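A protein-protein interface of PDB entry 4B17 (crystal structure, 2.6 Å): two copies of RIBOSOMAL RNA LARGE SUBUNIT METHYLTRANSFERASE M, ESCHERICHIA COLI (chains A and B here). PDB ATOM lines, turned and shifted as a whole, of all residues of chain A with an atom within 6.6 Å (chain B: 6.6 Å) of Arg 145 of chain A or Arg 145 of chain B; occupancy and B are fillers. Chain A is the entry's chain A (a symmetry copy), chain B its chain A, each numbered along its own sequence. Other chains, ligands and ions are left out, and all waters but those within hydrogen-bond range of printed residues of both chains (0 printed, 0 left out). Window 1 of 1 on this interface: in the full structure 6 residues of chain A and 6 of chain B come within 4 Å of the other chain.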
ATOM      1  N   VAL A  97     -13.777   9.196 -33.243  1.00  0.00           N
ATOM      2  CA  VAL A  97     -13.660   8.248 -32.130  1.00  0.00           C
ATOM      3  C   VAL A  97     -12.892   8.882 -30.962  1.00  0.00           C
ATOM      4  O   VAL A  97     -11.794   9.432 -31.154  1.00  0.00           O
ATOM      5  CB  VAL A  97     -12.921   6.942 -32.537  1.00  0.00           C
ATOM      6  CG1 VAL A  97     -12.753   6.024 -31.327  1.00  0.00           C
ATOM      7  CG2 VAL A  97     -13.649   6.220 -33.650  1.00  0.00           C
ATOM      8  N   GLU A  98     -13.468   8.813 -29.764  1.00  0.00           N
ATOM      9  CA  GLU A  98     -12.782   9.253 -28.549  1.00  0.00           C
ATOM     10  C   GLU A  98     -12.505   8.078 -27.611  1.00  0.00           C
ATOM     11  O   GLU A  98     -13.406   7.313 -27.272  1.00  0.00           O
ATOM     12  CB  GLU A  98     -13.592  10.322 -27.806  1.00  0.00           C
ATOM     13  CG  GLU A  98     -12.897  11.681 -27.681  1.00  0.00           C
ATOM     14  CD  GLU A  98     -13.443  12.709 -28.666  1.00  0.00           C
ATOM     15  OE1 GLU A  98     -14.458  12.407 -29.339  1.00  0.00           O
ATOM     16  OE2 GLU A  98     -12.863  13.815 -28.763  1.00  0.00           O
ATOM     17  N   LYS A  99     -11.251   7.960 -27.193  1.00  0.00           N
ATOM     18  CA  LYS A  99     -10.813   6.915 -26.283  1.00  0.00           C
ATOM     19  C   LYS A  99     -11.184   5.518 -26.790  1.00  0.00           C
ATOM     20  O   LYS A  99     -11.783   4.714 -26.063  1.00  0.00           O
ATOM     21  CB  LYS A  99     -11.354   7.168 -24.872  1.00  0.00           C
ATOM     22  CG  LYS A  99     -11.008   8.552 -24.326  1.00  0.00           C
ATOM     23  CD  LYS A  99      -9.525   8.670 -23.960  1.00  0.00           C
ATOM     24  CE  LYS A  99      -9.132  10.124 -23.679  1.00  0.00           C
ATOM     25  NZ  LYS A  99      -7.718  10.243 -23.203  1.00  0.00           N
ATOM     26  N   GLY A 100     -10.818   5.240 -28.041  1.00  0.00           N
ATOM     27  CA  GLY A 100     -10.967   3.916 -28.623  1.00  0.00           C
ATOM     28  C   GLY A 100     -10.185   2.847 -27.873  1.00  0.00           C
ATOM     29  O   GLY A 100      -9.255   3.148 -27.120  1.00  0.00           O
ATOM     30  N   GLY A 101     -10.561   1.590 -28.082  1.00  0.00           N
ATOM     31  CA  GLY A 101     -10.008   0.512 -27.301  1.00  0.00           C
ATOM     32  C   GLY A 101      -8.785  -0.154 -27.886  1.00  0.00           C
ATOM     33  O   GLY A 101      -8.010  -0.771 -27.152  1.00  0.00           O
ATOM     34  N   GLU A 102      -8.603  -0.040 -29.198  1.00  0.00           N
ATOM     35  CA  GLU A 102      -7.592  -0.833 -29.888  1.00  0.00           C
ATOM     36  C   GLU A 102      -7.383  -0.274 -31.286  1.00  0.00           C
ATOM     37  O   GLU A 102      -8.282   0.353 -31.852  1.00  0.00           O
ATOM     38  CB  GLU A 102      -8.056  -2.293 -29.980  1.00  0.00           C
ATOM     39  CG  GLU A 102      -6.971  -3.272 -30.362  1.00  0.00           C
ATOM     40  CD  GLU A 102      -7.498  -4.648 -30.770  1.00  0.00           C
ATOM     41  OE1 GLU A 102      -8.573  -5.067 -30.277  1.00  0.00           O
ATOM     42  OE2 GLU A 102      -6.817  -5.319 -31.580  1.00  0.00           O
ATOM     43  N   ALA A 138      -7.588   5.128 -26.060  1.00  0.00           N
ATOM     44  CA  ALA A 138      -7.341   5.110 -24.627  1.00  0.00           C
ATOM     45  C   ALA A 138      -5.878   4.722 -24.377  1.00  0.00           C
ATOM     46  O   ALA A 138      -5.248   4.084 -25.218  1.00  0.00           O
ATOM     47  CB  ALA A 138      -8.288   4.154 -23.936  1.00  0.00           C
ATOM     48  N   THR A 142      -8.558  -1.851 -24.433  1.00  0.00           N
ATOM     49  CA  THR A 142      -9.865  -2.153 -23.822  1.00  0.00           C
ATOM     50  C   THR A 142     -10.786  -2.887 -24.773  1.00  0.00           C
ATOM     51  O   THR A 142     -10.999  -2.440 -25.896  1.00  0.00           O
ATOM     52  CB  THR A 142     -10.663  -0.885 -23.392  1.00  0.00           C
ATOM     53  OG1 THR A 142      -9.786   0.147 -22.925  1.00  0.00           O
ATOM     54  CG2 THR A 142     -11.664  -1.237 -22.303  1.00  0.00           C
ATOM     55  N   PRO A 143     -11.372  -4.000 -24.313  1.00  0.00           N
ATOM     56  CA  PRO A 143     -12.406  -4.751 -25.042  1.00  0.00           C
ATOM     57  C   PRO A 143     -13.680  -3.947 -25.272  1.00  0.00           C
ATOM     58  O   PRO A 143     -14.297  -4.077 -26.322  1.00  0.00           O
ATOM     59  CB  PRO A 143     -12.727  -5.916 -24.098  1.00  0.00           C
ATOM     60  CG  PRO A 143     -11.519  -6.046 -23.210  1.00  0.00           C
ATOM     61  CD  PRO A 143     -10.992  -4.656 -23.049  1.00  0.00           C
ATOM     62  N   LYS A 144     -14.069  -3.123 -24.305  1.00  0.00           N
ATOM     63  CA  LYS A 144     -15.355  -2.440 -24.377  1.00  0.00           C
ATOM     64  C   LYS A 144     -15.319  -1.032 -24.968  1.00  0.00           C
ATOM     65  O   LYS A 144     -16.193  -0.213 -24.683  1.00  0.00           O
ATOM     66  CB  LYS A 144     -16.040  -2.425 -23.003  1.00  0.00           C
ATOM     67  CG  LYS A 144     -16.789  -3.728 -22.664  1.00  0.00           C
ATOM     68  CD  LYS A 144     -17.627  -3.609 -21.385  1.00  0.00           C
ATOM     69  CE  LYS A 144     -18.646  -4.741 -21.293  1.00  0.00           C
ATOM     70  NZ  LYS A 144     -19.518  -4.652 -20.087  1.00  0.00           N
ATOM     71  N   ARG A 145     -14.318  -0.740 -25.787  1.00  0.00           N
ATOM     72  CA  ARG A 145     -14.384   0.452 -26.628  1.00  0.00           C
ATOM     73  C   ARG A 145     -14.264  -0.016 -28.081  1.00  0.00           C
ATOM     74  O   ARG A 145     -13.819  -1.138 -28.329  1.00  0.00           O
ATOM     75  CB  ARG A 145     -13.300   1.471 -26.244  1.00  0.00           C
ATOM     76  CG  ARG A 145     -13.388   1.973 -24.809  1.00  0.00           C
ATOM     77  CD  ARG A 145     -14.612   2.856 -24.594  1.00  0.00           C
ATOM     78  NE  ARG A 145     -14.579   4.004 -25.485  1.00  0.00           N
ATOM     79  CZ  ARG A 145     -15.599   4.389 -26.239  1.00  0.00           C
ATOM     80  NH1 ARG A 145     -16.740   3.718 -26.188  1.00  0.00           N
ATOM     81  NH2 ARG A 145     -15.480   5.446 -27.036  1.00  0.00           N
ATOM     82  N   PRO A 146     -14.691   0.819 -29.045  1.00  0.00           N
ATOM     83  CA  PRO A 146     -14.642   0.351 -30.436  1.00  0.00           C
ATOM     84  C   PRO A 146     -13.215   0.078 -30.890  1.00  0.00           C
ATOM     85  O   PRO A 146     -12.289   0.705 -30.395  1.00  0.00           O
ATOM     86  CB  PRO A 146     -15.215   1.536 -31.230  1.00  0.00           C
ATOM     87  CG  PRO A 146     -16.010   2.309 -30.250  1.00  0.00           C
ATOM     88  CD  PRO A 146     -15.289   2.160 -28.935  1.00  0.00           C
ATOM     89  N   VAL A 147     -13.044  -0.850 -31.819  1.00  0.00           N
ATOM     90  CA  VAL A 147     -11.758  -1.032 -32.472  1.00  0.00           C
ATOM     91  C   VAL A 147     -11.596   0.091 -33.489  1.00  0.00           C
ATOM     92  O   VAL A 147     -12.528   0.380 -34.243  1.00  0.00           O
ATOM     93  CB  VAL A 147     -11.687  -2.402 -33.200  1.00  0.00           C
ATOM     94  CG1 VAL A 147     -10.416  -2.513 -34.007  1.00  0.00           C
ATOM     95  CG2 VAL A 147     -11.810  -3.551 -32.208  1.00  0.00           C
ATOM     96  N   VAL A 148     -10.430   0.735 -33.499  1.00  0.00           N
ATOM     97  CA  VAL A 148     -10.134   1.748 -34.518  1.00  0.00           C
ATOM     98  C   VAL A 148      -9.383   1.100 -35.682  1.00  0.00           C
ATOM     99  O   VAL A 148      -8.343   0.465 -35.487  1.00  0.00           O
ATOM    100  CB  VAL A 148      -9.297   2.934 -33.967  1.00  0.00           C
ATOM    101  CG1 VAL A 148      -8.955   3.917 -35.082  1.00  0.00           C
ATOM    102  CG2 VAL A 148     -10.036   3.643 -32.844  1.00  0.00           C
ATOM    103  N   SER A 163     -15.156  -0.272 -35.595  1.00  0.00           N
ATOM    104  CA  SER A 163     -16.163  -1.309 -35.459  1.00  0.00           C
ATOM    105  C   SER A 163     -16.350  -1.623 -33.972  1.00  0.00           C
ATOM    106  O   SER A 163     -15.493  -1.296 -33.136  1.00  0.00           O
ATOM    107  CB  SER A 163     -15.799  -2.562 -36.265  1.00  0.00           C
ATOM    108  OG  SER A 163     -14.759  -3.287 -35.647  1.00  0.00           O
ATOM    109  N   TYR A 164     -17.479  -2.233 -33.642  1.00  0.00           N
ATOM    110  CA  TYR A 164     -17.782  -2.564 -32.250  1.00  0.00           C
ATOM    111  C   TYR A 164     -17.261  -3.942 -31.928  1.00  0.00           C
ATOM    112  O   TYR A 164     -17.508  -4.880 -32.675  1.00  0.00           O
ATOM    113  CB  TYR A 164     -19.283  -2.458 -31.984  1.00  0.00           C
ATOM    114  CG  TYR A 164     -19.788  -1.055 -32.212  1.00  0.00           C
ATOM    115  CD1 TYR A 164     -19.608  -0.070 -31.245  1.00  0.00           C
ATOM    116  CD2 TYR A 164     -20.411  -0.702 -33.402  1.00  0.00           C
ATOM    117  CE1 TYR A 164     -20.048   1.234 -31.452  1.00  0.00           C
ATOM    118  CE2 TYR A 164     -20.853   0.601 -33.620  1.00  0.00           C
ATOM    119  CZ  TYR A 164     -20.667   1.564 -32.637  1.00  0.00           C
ATOM    120  OH  TYR A 164     -21.105   2.860 -32.834  1.00  0.00           O
ATOM    121  N   SER A 165     -16.521  -4.053 -30.825  1.00  0.00           N
ATOM    122  CA  SER A 165     -15.893  -5.318 -30.434  1.00  0.00           C
ATOM    123  C   SER A 165     -16.895  -6.425 -30.126  1.00  0.00           C
ATOM    124  O   SER A 165     -16.564  -7.610 -30.242  1.00  0.00           O
ATOM    125  CB  SER A 165     -14.949  -5.129 -29.249  1.00  0.00           C
ATOM    126  OG  SER A 165     -15.570  -4.399 -28.210  1.00  0.00           O
ATOM    127  N   VAL B  97     -19.869   1.679 -17.728  1.00  0.00           N
ATOM    128  CA  VAL B  97     -19.265   2.782 -18.483  1.00  0.00           C
ATOM    129  C   VAL B  97     -17.737   2.642 -18.508  1.00  0.00           C
ATOM    130  O   VAL B  97     -17.102   2.466 -17.456  1.00  0.00           O
ATOM    131  CB  VAL B  97     -19.609   4.173 -17.880  1.00  0.00           C
ATOM    132  CG1 VAL B  97     -18.894   5.281 -18.650  1.00  0.00           C
ATOM    133  CG2 VAL B  97     -21.103   4.416 -17.870  1.00  0.00           C
ATOM    134  N   GLU B  98     -17.154   2.713 -19.703  1.00  0.00           N
ATOM    135  CA  GLU B  98     -15.698   2.734 -19.855  1.00  0.00           C
ATOM    136  C   GLU B  98     -15.218   4.072 -20.416  1.00  0.00           C
ATOM    137  O   GLU B  98     -15.704   4.538 -21.444  1.00  0.00           O
ATOM    138  CB  GLU B  98     -15.214   1.595 -20.760  1.00  0.00           C
ATOM    139  CG  GLU B  98     -14.286   0.586 -20.078  1.00  0.00           C
ATOM    140  CD  GLU B  98     -14.999  -0.713 -19.719  1.00  0.00           C
ATOM    141  OE1 GLU B  98     -16.171  -0.882 -20.133  1.00  0.00           O
ATOM    142  OE2 GLU B  98     -14.388  -1.564 -19.029  1.00  0.00           O
ATOM    143  N   LYS B  99     -14.252   4.668 -19.730  1.00  0.00           N
ATOM    144  CA  LYS B  99     -13.660   5.935 -20.129  1.00  0.00           C
ATOM    145  C   LYS B  99     -14.718   7.024 -20.332  1.00  0.00           C
ATOM    146  O   LYS B  99     -14.754   7.691 -21.375  1.00  0.00           O
ATOM    147  CB  LYS B  99     -12.787   5.754 -21.374  1.00  0.00           C
ATOM    148  CG  LYS B  99     -11.718   4.675 -21.217  1.00  0.00           C
ATOM    149  CD  LYS B  99     -10.587   5.120 -20.284  1.00  0.00           C
ATOM    150  CE  LYS B  99      -9.672   3.948 -19.916  1.00  0.00           C
ATOM    151  NZ  LYS B  99      -8.494   4.386 -19.103  1.00  0.00           N
ATOM    152  N   GLY B 100     -15.572   7.197 -19.323  1.00  0.00           N
ATOM    153  CA  GLY B 100     -16.542   8.280 -19.297  1.00  0.00           C
ATOM    154  C   GLY B 100     -15.894   9.657 -19.336  1.00  0.00           C
ATOM    155  O   GLY B 100     -14.708   9.812 -19.038  1.00  0.00           O
ATOM    156  N   GLY B 101     -16.680  10.665 -19.705  1.00  0.00           N
ATOM    157  CA  GLY B 101     -16.135  11.979 -19.941  1.00  0.00           C
ATOM    158  C   GLY B 101     -16.139  12.907 -18.750  1.00  0.00           C
ATOM    159  O   GLY B 101     -15.357  13.860 -18.710  1.00  0.00           O
ATOM    160  N   GLU B 102     -17.010  12.644 -17.780  1.00  0.00           N
ATOM    161  CA  GLU B 102     -17.253  13.603 -16.708  1.00  0.00           C
ATOM    162  C   GLU B 102     -18.026  12.922 -15.591  1.00  0.00           C
ATOM    163  O   GLU B 102     -18.743  11.948 -15.828  1.00  0.00           O
ATOM    164  CB  GLU B 102     -18.062  14.789 -17.249  1.00  0.00           C
ATOM    165  CG  GLU B 102     -18.089  15.996 -16.342  1.00  0.00           C
ATOM    166  CD  GLU B 102     -19.149  17.030 -16.723  1.00  0.00           C
ATOM    167  OE1 GLU B 102     -19.497  17.142 -17.923  1.00  0.00           O
ATOM    168  OE2 GLU B 102     -19.623  17.745 -15.809  1.00  0.00           O
ATOM    169  N   ALA B 138     -12.322   8.705 -18.085  1.00  0.00           N
ATOM    170  CA  ALA B 138     -11.092   9.041 -18.782  1.00  0.00           C
ATOM    171  C   ALA B 138     -10.230   9.930 -17.878  1.00  0.00           C
ATOM    172  O   ALA B 138     -10.745  10.593 -16.979  1.00  0.00           O
ATOM    173  CB  ALA B 138     -11.397   9.728 -20.096  1.00  0.00           C
ATOM    174  N   THR B 142     -13.927  15.130 -20.991  1.00  0.00           N
ATOM    175  CA  THR B 142     -14.271  15.075 -22.422  1.00  0.00           C
ATOM    176  C   THR B 142     -15.751  15.293 -22.664  1.00  0.00           C
ATOM    177  O   THR B 142     -16.581  14.620 -22.059  1.00  0.00           O
ATOM    178  CB  THR B 142     -13.955  13.703 -23.091  1.00  0.00           C
ATOM    179  OG1 THR B 142     -12.773  13.116 -22.536  1.00  0.00           O
ATOM    180  CG2 THR B 142     -13.782  13.877 -24.592  1.00  0.00           C
ATOM    181  N   PRO B 143     -16.087  16.207 -23.583  1.00  0.00           N
ATOM    182  CA  PRO B 143     -17.463  16.439 -24.052  1.00  0.00           C
ATOM    183  C   PRO B 143     -18.068  15.230 -24.754  1.00  0.00           C
ATOM    184  O   PRO B 143     -19.255  14.971 -24.602  1.00  0.00           O
ATOM    185  CB  PRO B 143     -17.301  17.570 -25.075  1.00  0.00           C
ATOM    186  CG  PRO B 143     -16.002  18.240 -24.716  1.00  0.00           C
ATOM    187  CD  PRO B 143     -15.127  17.152 -24.181  1.00  0.00           C
ATOM    188  N   LYS B 144     -17.263  14.496 -25.516  1.00  0.00           N
ATOM    189  CA  LYS B 144     -17.793  13.421 -26.346  1.00  0.00           C
ATOM    190  C   LYS B 144     -17.759  12.029 -25.720  1.00  0.00           C
ATOM    191  O   LYS B 144     -17.744  11.025 -26.433  1.00  0.00           O
ATOM    192  CB  LYS B 144     -17.106  13.407 -27.720  1.00  0.00           C
ATOM    193  CG  LYS B 144     -17.689  14.423 -28.720  1.00  0.00           C
ATOM    194  CD  LYS B 144     -17.124  14.245 -30.135  1.00  0.00           C
ATOM    195  CE  LYS B 144     -17.987  14.972 -31.163  1.00  0.00           C
ATOM    196  NZ  LYS B 144     -17.507  14.798 -32.563  1.00  0.00           N
ATOM    197  N   ARG B 145     -17.744  11.956 -24.397  1.00  0.00           N
ATOM    198  CA  ARG B 145     -18.029  10.688 -23.730  1.00  0.00           C
ATOM    199  C   ARG B 145     -19.236  10.921 -22.817  1.00  0.00           C
ATOM    200  O   ARG B 145     -19.557  12.070 -22.507  1.00  0.00           O
ATOM    201  CB  ARG B 145     -16.803  10.167 -22.966  1.00  0.00           C
ATOM    202  CG  ARG B 145     -15.580   9.909 -23.837  1.00  0.00           C
ATOM    203  CD  ARG B 145     -15.790   8.717 -24.765  1.00  0.00           C
ATOM    204  NE  ARG B 145     -16.074   7.514 -23.998  1.00  0.00           N
ATOM    205  CZ  ARG B 145     -17.083   6.693 -24.252  1.00  0.00           C
ATOM    206  NH1 ARG B 145     -17.890   6.944 -25.271  1.00  0.00           N
ATOM    207  NH2 ARG B 145     -17.277   5.619 -23.493  1.00  0.00           N
ATOM    208  N   PRO B 146     -19.932   9.845 -22.411  1.00  0.00           N
ATOM    209  CA  PRO B 146     -21.130  10.066 -21.592  1.00  0.00           C
ATOM    210  C   PRO B 146     -20.790  10.718 -20.260  1.00  0.00           C
ATOM    211  O   PRO B 146     -19.695  10.527 -19.750  1.00  0.00           O
ATOM    212  CB  PRO B 146     -21.659   8.643 -21.345  1.00  0.00           C
ATOM    213  CG  PRO B 146     -21.082   7.823 -22.434  1.00  0.00           C
ATOM    214  CD  PRO B 146     -19.728   8.419 -22.717  1.00  0.00           C
ATOM    215  N   VAL B 147     -21.720  11.484 -19.708  1.00  0.00           N
ATOM    216  CA  VAL B 147     -21.581  11.973 -18.346  1.00  0.00           C
ATOM    217  C   VAL B 147     -21.899  10.816 -17.406  1.00  0.00           C
ATOM    218  O   VAL B 147     -22.891  10.112 -17.609  1.00  0.00           O
ATOM    219  CB  VAL B 147     -22.557  13.147 -18.068  1.00  0.00           C
ATOM    220  CG1 VAL B 147     -22.520  13.540 -16.610  1.00  0.00           C
ATOM    221  CG2 VAL B 147     -22.244  14.337 -18.966  1.00  0.00           C
ATOM    222  N   VAL B 148     -21.055  10.605 -16.397  1.00  0.00           N
ATOM    223  CA  VAL B 148     -21.339   9.594 -15.373  1.00  0.00           C
ATOM    224  C   VAL B 148     -22.039  10.253 -14.183  1.00  0.00           C
ATOM    225  O   VAL B 148     -21.533  11.221 -13.610  1.00  0.00           O
ATOM    226  CB  VAL B 148     -20.063   8.863 -14.874  1.00  0.00           C
ATOM    227  CG1 VAL B 148     -20.407   7.880 -13.759  1.00  0.00           C
ATOM    228  CG2 VAL B 148     -19.368   8.146 -16.019  1.00  0.00           C
ATOM    229  N   SER B 163     -25.583   9.619 -18.901  1.00  0.00           N
ATOM    230  CA  SER B 163     -26.374  10.268 -19.931  1.00  0.00           C
ATOM    231  C   SER B 163     -25.438  10.744 -21.045  1.00  0.00           C
ATOM    232  O   SER B 163     -24.219  10.864 -20.850  1.00  0.00           O
ATOM    233  CB  SER B 163     -27.212  11.419 -19.360  1.00  0.00           C
ATOM    234  OG  SER B 163     -26.411  12.541 -19.063  1.00  0.00           O
ATOM    235  N   TYR B 164     -26.004  10.988 -22.218  1.00  0.00           N
ATOM    236  CA  TYR B 164     -25.210  11.425 -23.365  1.00  0.00           C
ATOM    237  C   TYR B 164     -25.138  12.931 -23.393  1.00  0.00           C
ATOM    238  O   TYR B 164     -26.159  13.596 -23.276  1.00  0.00           O
ATOM    239  CB  TYR B 164     -25.791  10.870 -24.666  1.00  0.00           C
ATOM    240  CG  TYR B 164     -25.775   9.362 -24.681  1.00  0.00           C
ATOM    241  CD1 TYR B 164     -24.606   8.668 -24.978  1.00  0.00           C
ATOM    242  CD2 TYR B 164     -26.912   8.629 -24.366  1.00  0.00           C
ATOM    243  CE1 TYR B 164     -24.570   7.277 -24.971  1.00  0.00           C
ATOM    244  CE2 TYR B 164     -26.887   7.237 -24.355  1.00  0.00           C
ATOM    245  CZ  TYR B 164     -25.709   6.568 -24.661  1.00  0.00           C
ATOM    246  OH  TYR B 164     -25.668   5.187 -24.661  1.00  0.00           O
ATOM    247  N   SER B 165     -23.923  13.463 -23.525  1.00  0.00           N
ATOM    248  CA  SER B 165     -23.701  14.910 -23.493  1.00  0.00           C
ATOM    249  C   SER B 165     -24.380  15.655 -24.636  1.00  0.00           C
ATOM    250  O   SER B 165     -24.683  16.846 -24.506  1.00  0.00           O
ATOM    251  CB  SER B 165     -22.211  15.246 -23.468  1.00  0.00           C
ATOM    252  OG  SER B 165     -21.508  14.534 -24.467  1.00  0.00           O
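CG of Glu 98 of chain A touches CG2 of Thr 142 of chain B, at 3.9 Å. OE1 of Glu 98 of chain A touches CB of Lys 144 of chain B, at 3.3 Å. O of Glu 98 of chain A touches CD of Arg 145 of chain B (3.7 Å). CG2 of Thr 142 of chain A touches CG of Glu 98 of chain B (3.9 Å). Lys 144 of chain A touches Glu 98 of chain B. O of Glu 98 of chain B touches CD of Arg 145 of chain A, 3.7 Å away.
Of the printed residues of chain B, Glu 98 of chain A touches Thr 142 (3.9 Å), Lys 144 (3.3 Å) and Arg 145 (3.7 Å). Printed residues of chain B within 4 Å of Thr 142 of chain A: Glu 98. Printed residues of chain B within 4 Å of Lys 144 of chain A: Glu 98. Arg 145 of chain A touches just these residues of chain B: Glu 98 (3.7 Å) and Arg 145 (3.3 Å). Printed residues of chain A within 4 Å of Glu 98 of chain B: Thr 142, Lys 144 and Arg 145. Printed residues of chain A within 4 Å of Lys 144 of chain B: Glu 98. Of chain A, only Glu 98 and Arg 145 come within 4 Å of Arg 145 of chain B. The nearest residue of chain B that does not touch Arg 145 of chain A is Lys 99 of chain B (4.7 Å). The nearest residue of chain A that does not touch Arg 145 of chain B is Lys 99 of chain A (4.7 Å).
Of the 17 printed residues of chain A, 4 touch a printed residue of chain B. Printed residues of chain A that touch a printed residue of chain B: Glu 98, Thr 142, Lys 144 and Arg 145. Among the printed residues, 7 pairs touch across the chains. Among the printed residues, no Asp or Glu carboxylate lies within 4 Å of a Lys or Arg side-chain nitrogen of the other chain.
The guanidinium group of Arg 145 of chain B sits close to the guanidinium group of Arg 145 of chain A, 3.3 Å away.
Glu 98 of chain A touches Thr 142 of chain B, and with the chains exchanged Thr 142 of chain A touches Glu 98 of chain B. Glu 98 of chain A touches Lys 144 of chain B, and with the chains exchanged Lys 144 of chain A touches Glu 98 of chain B. Glu 98 of chain A touches Arg 145 of chain B, and with the chains exchanged Arg 145 of chain A touches Glu 98 of chain B. Arg 145 of chain B touches its own counterpart, Arg 145 of chain A. Positions printed for both chains: 97, 98, 99, 100, 101, 102, 138, 142, 143, 144, 145, 146, 147, 148, 163, 164 and 165.
The guanidinium group of Arg 145 of chain B lies within hydrogen-bond range of the backbone carbonyl oxygen of Glu 98 of chain B (2.8 Å). O of Lys 99 of chain B lies within hydrogen-bond range of NE of Arg 145 of chain B, at 2.9 Å. The backbone carbonyl oxygen (O) of Gly 101 of chain B lies within hydrogen-bond range of the backbone NH (N) of Thr 142 of chain B, at 3.0 Å. O of Glu 98 of chain A lies within hydrogen-bond range of NH2 of Arg 145 of chain A (2.8 Å). O of Lys 99 of chain A is in hydrogen-bond range of NE of Arg 145 of chain A (2.9 Å). N of Thr 142 of chain A is in hydrogen-bond range of O of Gly 101 of chain A, at 3.0 Å.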
